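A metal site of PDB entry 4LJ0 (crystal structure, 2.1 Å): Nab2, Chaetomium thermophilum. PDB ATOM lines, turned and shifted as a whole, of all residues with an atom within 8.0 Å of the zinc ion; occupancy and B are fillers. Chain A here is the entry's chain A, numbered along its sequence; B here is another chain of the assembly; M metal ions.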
ATOM      1  N   PRO A  24      10.504 -21.617 -20.563  1.00  0.00           N
ATOM      2  CA  PRO A  24      10.347 -21.486 -19.108  1.00  0.00           C
ATOM      3  C   PRO A  24      10.887 -22.715 -18.401  1.00  0.00           C
ATOM      4  O   PRO A  24      11.012 -23.773 -19.030  1.00  0.00           O
ATOM      5  CB  PRO A  24       8.829 -21.386 -18.906  1.00  0.00           C
ATOM      6  CG  PRO A  24       8.234 -21.212 -20.257  1.00  0.00           C
ATOM      7  CD  PRO A  24       9.202 -21.765 -21.241  1.00  0.00           C
ATOM      8  N   PRO A  25      11.204 -22.605 -17.107  1.00  0.00           N
ATOM      9  CA  PRO A  25      11.711 -23.759 -16.359  1.00  0.00           C
ATOM     10  C   PRO A  25      10.629 -24.814 -16.192  1.00  0.00           C
ATOM     11  O   PRO A  25       9.458 -24.472 -16.057  1.00  0.00           O
ATOM     12  CB  PRO A  25      12.096 -23.151 -15.006  1.00  0.00           C
ATOM     13  CG  PRO A  25      11.193 -21.965 -14.867  1.00  0.00           C
ATOM     14  CD  PRO A  25      11.021 -21.418 -16.247  1.00  0.00           C
ATOM     15  N   CYS A  26      11.011 -26.089 -16.222  1.00  0.00           N
ATOM     16  CA  CYS A  26      10.040 -27.168 -16.039  1.00  0.00           C
ATOM     17  C   CYS A  26       9.611 -27.263 -14.586  1.00  0.00           C
ATOM     18  O   CYS A  26      10.456 -27.405 -13.703  1.00  0.00           O
ATOM     19  CB  CYS A  26      10.612 -28.504 -16.494  1.00  0.00           C
ATOM     20  SG  CYS A  26       9.406 -29.845 -16.391  1.00  0.00           S
ATOM     21  N   ARG A  27       8.305 -27.191 -14.337  1.00  0.00           N
ATOM     22  CA  ARG A  27       7.766 -27.254 -12.989  1.00  0.00           C
ATOM     23  C   ARG A  27       7.681 -28.678 -12.445  1.00  0.00           C
ATOM     24  O   ARG A  27       7.200 -28.894 -11.335  1.00  0.00           O
ATOM     25  CB  ARG A  27       6.379 -26.609 -12.921  1.00  0.00           C
ATOM     26  CG  ARG A  27       6.337 -25.109 -13.149  1.00  0.00           C
ATOM     27  CD  ARG A  27       5.012 -24.553 -12.627  1.00  0.00           C
ATOM     28  NE  ARG A  27       4.576 -23.334 -13.317  1.00  0.00           N
ATOM     29  CZ  ARG A  27       4.977 -22.106 -13.008  1.00  0.00           C
ATOM     30  NH1 ARG A  27       5.839 -21.911 -12.026  1.00  0.00           N
ATOM     31  NH2 ARG A  27       4.510 -21.074 -13.690  1.00  0.00           N
ATOM     32  N   ASN A  28       8.132 -29.666 -13.232  1.00  0.00           N
ATOM     33  CA  ASN A  28       8.294 -31.027 -12.726  1.00  0.00           C
ATOM     34  C   ASN A  28       9.631 -31.200 -12.026  1.00  0.00           C
ATOM     35  O   ASN A  28       9.909 -32.250 -11.445  1.00  0.00           O
ATOM     36  CB  ASN A  28       8.196 -32.053 -13.857  1.00  0.00           C
ATOM     37  CG  ASN A  28       6.809 -32.149 -14.465  1.00  0.00           C
ATOM     38  OD1 ASN A  28       5.812 -31.858 -13.815  1.00  0.00           O
ATOM     39  ND2 ASN A  28       6.744 -32.580 -15.725  1.00  0.00           N
ATOM     40  N   GLY A  29      10.473 -30.170 -12.106  1.00  0.00           N
ATOM     41  CA  GLY A  29      11.825 -30.231 -11.558  1.00  0.00           C
ATOM     42  C   GLY A  29      12.840 -30.605 -12.621  1.00  0.00           C
ATOM     43  O   GLY A  29      12.491 -31.027 -13.724  1.00  0.00           O
ATOM     44  N   GLY A  30      14.128 -30.443 -12.286  1.00  0.00           N
ATOM     45  CA  GLY A  30      15.195 -30.798 -13.191  1.00  0.00           C
ATOM     46  C   GLY A  30      15.209 -32.288 -13.494  1.00  0.00           C
ATOM     47  O   GLY A  30      15.704 -32.718 -14.532  1.00  0.00           O
ATOM     48  N   GLU A  31      14.643 -33.084 -12.583  1.00  0.00           N
ATOM     49  CA  GLU A  31      14.657 -34.544 -12.720  1.00  0.00           C
ATOM     50  C   GLU A  31      13.477 -35.070 -13.545  1.00  0.00           C
ATOM     51  O   GLU A  31      13.261 -36.281 -13.613  1.00  0.00           O
ATOM     52  CB  GLU A  31      14.682 -35.218 -11.342  1.00  0.00           C
ATOM     53  CG  GLU A  31      13.364 -35.193 -10.562  1.00  0.00           C
ATOM     54  CD  GLU A  31      13.103 -33.889  -9.828  1.00  0.00           C
ATOM     55  OE1 GLU A  31      13.835 -32.903 -10.045  1.00  0.00           O
ATOM     56  OE2 GLU A  31      12.150 -33.858  -9.016  1.00  0.00           O
ATOM     57  N   CYS A  32      12.713 -34.165 -14.149  1.00  0.00           N
ATOM     58  CA  CYS A  32      11.558 -34.507 -14.990  1.00  0.00           C
ATOM     59  C   CYS A  32      11.913 -35.603 -15.993  1.00  0.00           C
ATOM     60  O   CYS A  32      12.888 -35.452 -16.743  1.00  0.00           O
ATOM     61  CB  CYS A  32      11.081 -33.263 -15.745  1.00  0.00           C
ATOM     62  SG  CYS A  32       9.761 -33.505 -16.995  1.00  0.00           S
ATOM     63  N   LYS A  33      11.152 -36.687 -15.991  1.00  0.00           N
ATOM     64  CA  LYS A  33      11.372 -37.798 -16.921  1.00  0.00           C
ATOM     65  C   LYS A  33      10.261 -37.910 -17.964  1.00  0.00           C
ATOM     66  O   LYS A  33      10.152 -38.926 -18.643  1.00  0.00           O
ATOM     67  CB  LYS A  33      11.443 -39.129 -16.174  1.00  0.00           C
ATOM     68  CG  LYS A  33      12.398 -39.162 -15.010  1.00  0.00           C
ATOM     69  CD  LYS A  33      13.831 -39.025 -15.451  1.00  0.00           C
ATOM     70  CE  LYS A  33      14.801 -39.469 -14.364  1.00  0.00           C
ATOM     71  NZ  LYS A  33      15.065 -38.389 -13.362  1.00  0.00           N
ATOM     72  N   VAL A  34       9.427 -36.885 -18.079  1.00  0.00           N
ATOM     73  CA  VAL A  34       8.333 -36.916 -19.044  1.00  0.00           C
ATOM     74  C   VAL A  34       8.902 -36.885 -20.465  1.00  0.00           C
ATOM     75  O   VAL A  34       9.652 -35.987 -20.821  1.00  0.00           O
ATOM     76  CB  VAL A  34       7.363 -35.725 -18.835  1.00  0.00           C
ATOM     77  CG1 VAL A  34       6.293 -35.706 -19.916  1.00  0.00           C
ATOM     78  CG2 VAL A  34       6.719 -35.799 -17.450  1.00  0.00           C
ATOM     79  N   PRO A  35       8.559 -37.898 -21.293  1.00  0.00           N
ATOM     80  CA  PRO A  35       9.045 -37.893 -22.674  1.00  0.00           C
ATOM     81  C   PRO A  35       8.531 -36.704 -23.476  1.00  0.00           C
ATOM     82  O   PRO A  35       7.353 -36.362 -23.374  1.00  0.00           O
ATOM     83  CB  PRO A  35       8.464 -39.187 -23.265  1.00  0.00           C
ATOM     84  CG  PRO A  35       8.129 -40.040 -22.088  1.00  0.00           C
ATOM     85  CD  PRO A  35       7.755 -39.101 -20.994  1.00  0.00           C
ATOM     86  N   GLY A  36       9.405 -36.087 -24.267  1.00  0.00           N
ATOM     87  CA  GLY A  36       9.005 -34.977 -25.115  1.00  0.00           C
ATOM     88  C   GLY A  36       8.952 -33.623 -24.414  1.00  0.00           C
ATOM     89  O   GLY A  36       8.717 -32.608 -25.065  1.00  0.00           O
ATOM     90  N   CYS A  37       9.163 -33.595 -23.099  1.00  0.00           N
ATOM     91  CA  CYS A  37       9.140 -32.333 -22.370  1.00  0.00           C
ATOM     92  C   CYS A  37      10.341 -31.494 -22.773  1.00  0.00           C
ATOM     93  O   CYS A  37      11.486 -31.914 -22.609  1.00  0.00           O
ATOM     94  CB  CYS A  37       9.144 -32.574 -20.854  1.00  0.00           C
ATOM     95  SG  CYS A  37       9.024 -31.048 -19.841  1.00  0.00           S
ATOM     96  N   LYS A  38      10.077 -30.298 -23.302  1.00  0.00           N
ATOM     97  CA  LYS A  38      11.135 -29.405 -23.795  1.00  0.00           C
ATOM     98  C   LYS A  38      11.192 -28.116 -22.990  1.00  0.00           C
ATOM     99  O   LYS A  38      11.782 -27.131 -23.446  1.00  0.00           O
ATOM    100  CB  LYS A  38      10.897 -29.068 -25.273  1.00  0.00           C
ATOM    101  CG  LYS A  38      10.882 -30.266 -26.192  1.00  0.00           C
ATOM    102  CD  LYS A  38      12.245 -30.928 -26.289  1.00  0.00           C
ATOM    103  CE  LYS A  38      12.251 -32.011 -27.352  1.00  0.00           C
ATOM    104  NZ  LYS A  38      13.628 -32.545 -27.592  1.00  0.00           N
ATOM    105  N   PHE A  39      10.583 -28.093 -21.817  1.00  0.00           N
ATOM    106  CA  PHE A  39      10.772 -26.976 -20.923  1.00  0.00           C
ATOM    107  C   PHE A  39      12.218 -27.018 -20.456  1.00  0.00           C
ATOM    108  O   PHE A  39      12.872 -28.046 -20.601  1.00  0.00           O
ATOM    109  CB  PHE A  39       9.811 -27.053 -19.741  1.00  0.00           C
ATOM    110  CG  PHE A  39       8.384 -26.738 -20.106  1.00  0.00           C
ATOM    111  CD1 PHE A  39       7.976 -25.422 -20.293  1.00  0.00           C
ATOM    112  CD2 PHE A  39       7.445 -27.740 -20.251  1.00  0.00           C
ATOM    113  CE1 PHE A  39       6.671 -25.125 -20.625  1.00  0.00           C
ATOM    114  CE2 PHE A  39       6.130 -27.450 -20.575  1.00  0.00           C
ATOM    115  CZ  PHE A  39       5.744 -26.138 -20.764  1.00  0.00           C
ATOM    116  N   THR A  40      12.738 -25.919 -19.922  1.00  0.00           N
ATOM    117  CA  THR A  40      14.121 -25.905 -19.476  1.00  0.00           C
ATOM    118  C   THR A  40      14.245 -26.694 -18.186  1.00  0.00           C
ATOM    119  O   THR A  40      13.584 -26.396 -17.198  1.00  0.00           O
ATOM    120  CB  THR A  40      14.620 -24.471 -19.240  1.00  0.00           C
ATOM    121  OG1 THR A  40      14.419 -23.694 -20.424  1.00  0.00           O
ATOM    122  CG2 THR A  40      16.110 -24.477 -18.888  1.00  0.00           C
ATOM    123  N   HIS A  41      15.097 -27.709 -18.211  1.00  0.00           N
ATOM    124  CA  HIS A  41      15.339 -28.513 -17.023  1.00  0.00           C
ATOM    125  C   HIS A  41      16.625 -28.068 -16.338  1.00  0.00           C
ATOM    126  O   HIS A  41      17.706 -28.170 -16.909  1.00  0.00           O
ATOM    127  CB  HIS A  41      15.395 -29.997 -17.406  1.00  0.00           C
ATOM    128  CG  HIS A  41      14.106 -30.496 -17.977  1.00  0.00           C
ATOM    129  ND1 HIS A  41      13.905 -30.627 -19.333  1.00  0.00           N
ATOM    130  CD2 HIS A  41      12.943 -30.850 -17.391  1.00  0.00           C
ATOM    131  CE1 HIS A  41      12.676 -31.067 -19.549  1.00  0.00           C
ATOM    132  NE2 HIS A  41      12.078 -31.222 -18.386  1.00  0.00           N
ATOM    133  P     A B   2       2.691 -18.940 -17.494  1.00  0.00           P
ATOM    134  OP1   A B   2       1.239 -18.640 -17.538  1.00  0.00           O
ATOM    135  OP2   A B   2       3.643 -17.880 -17.074  1.00  0.00           O
ATOM    136  O5'   A B   2       2.903 -20.209 -16.549  1.00  0.00           O
ATOM    137  C5'   A B   2       3.713 -21.292 -16.974  1.00  0.00           C
ATOM    138  C4'   A B   2       2.961 -22.262 -17.841  1.00  0.00           C
ATOM    139  O4'   A B   2       3.841 -23.353 -18.226  1.00  0.00           O
ATOM    140  C3'   A B   2       1.738 -22.906 -17.188  1.00  0.00           C
ATOM    141  O3'   A B   2       0.712 -23.124 -18.162  1.00  0.00           O
ATOM    142  C2'   A B   2       2.286 -24.243 -16.707  1.00  0.00           C
ATOM    143  O2'   A B   2       1.318 -25.253 -16.543  1.00  0.00           O
ATOM    144  C1'   A B   2       3.283 -24.583 -17.804  1.00  0.00           C
ATOM    145  N9    A B   2       4.371 -25.463 -17.393  1.00  0.00           N
ATOM    146  C8    A B   2       5.575 -25.148 -16.803  1.00  0.00           C
ATOM    147  N7    A B   2       6.333 -26.186 -16.557  1.00  0.00           N
ATOM    148  C5    A B   2       5.580 -27.264 -17.022  1.00  0.00           C
ATOM    149  C6    A B   2       5.817 -28.648 -17.060  1.00  0.00           C
ATOM    150  N6    A B   2       6.925 -29.232 -16.603  1.00  0.00           N
ATOM    151  N1    A B   2       4.855 -29.435 -17.593  1.00  0.00           N
ATOM    152  C2    A B   2       3.730 -28.868 -18.047  1.00  0.00           C
ATOM    153  N3    A B   2       3.398 -27.578 -18.068  1.00  0.00           N
ATOM    154  C4    A B   2       4.375 -26.829 -17.547  1.00  0.00           C
HETATM  155 ZN    ZN M   1      10.059 -31.426 -17.920  1.00  0.00          ZN
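Of the 19 residues printed, 4 come within 4 Å of the zinc ion. The nearest printed residue that does not touch the zinc ion is A 2 of chain B (4.05 Å).
The zinc ion is bound by a ring nitrogen (NE2) of His 41 (2.1 Å), the side-chain sulfur (SG) of Cys 37 (2.2 Å), the side-chain sulfur (SG) of Cys 26 (2.3 Å) and the side-chain sulfur (SG) of Cys 32 (2.3 Å). The zinc ion has four donor atoms within binding distance.
A ring nitrogen (ND1) of His 41 lies within hydrogen-bond range of the backbone carbonyl oxygen (O) of Phe 39 (3.1 Å). SG of Cys 26 sits close to N6 of A 2 of chain B (2.6 Å). SG of Cys 26 sits close to N of Asn 28 (3.4 Å). The backbone NH (N) of Cys 26 is in hydrogen-bond range of the backbone carbonyl oxygen (O) of Thr 40, 2.8 Å away. SG of Cys 32 sits close to ND2 of Asn 28. N of Val 34 lies close to SG of Cys 32 (3.6 Å).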
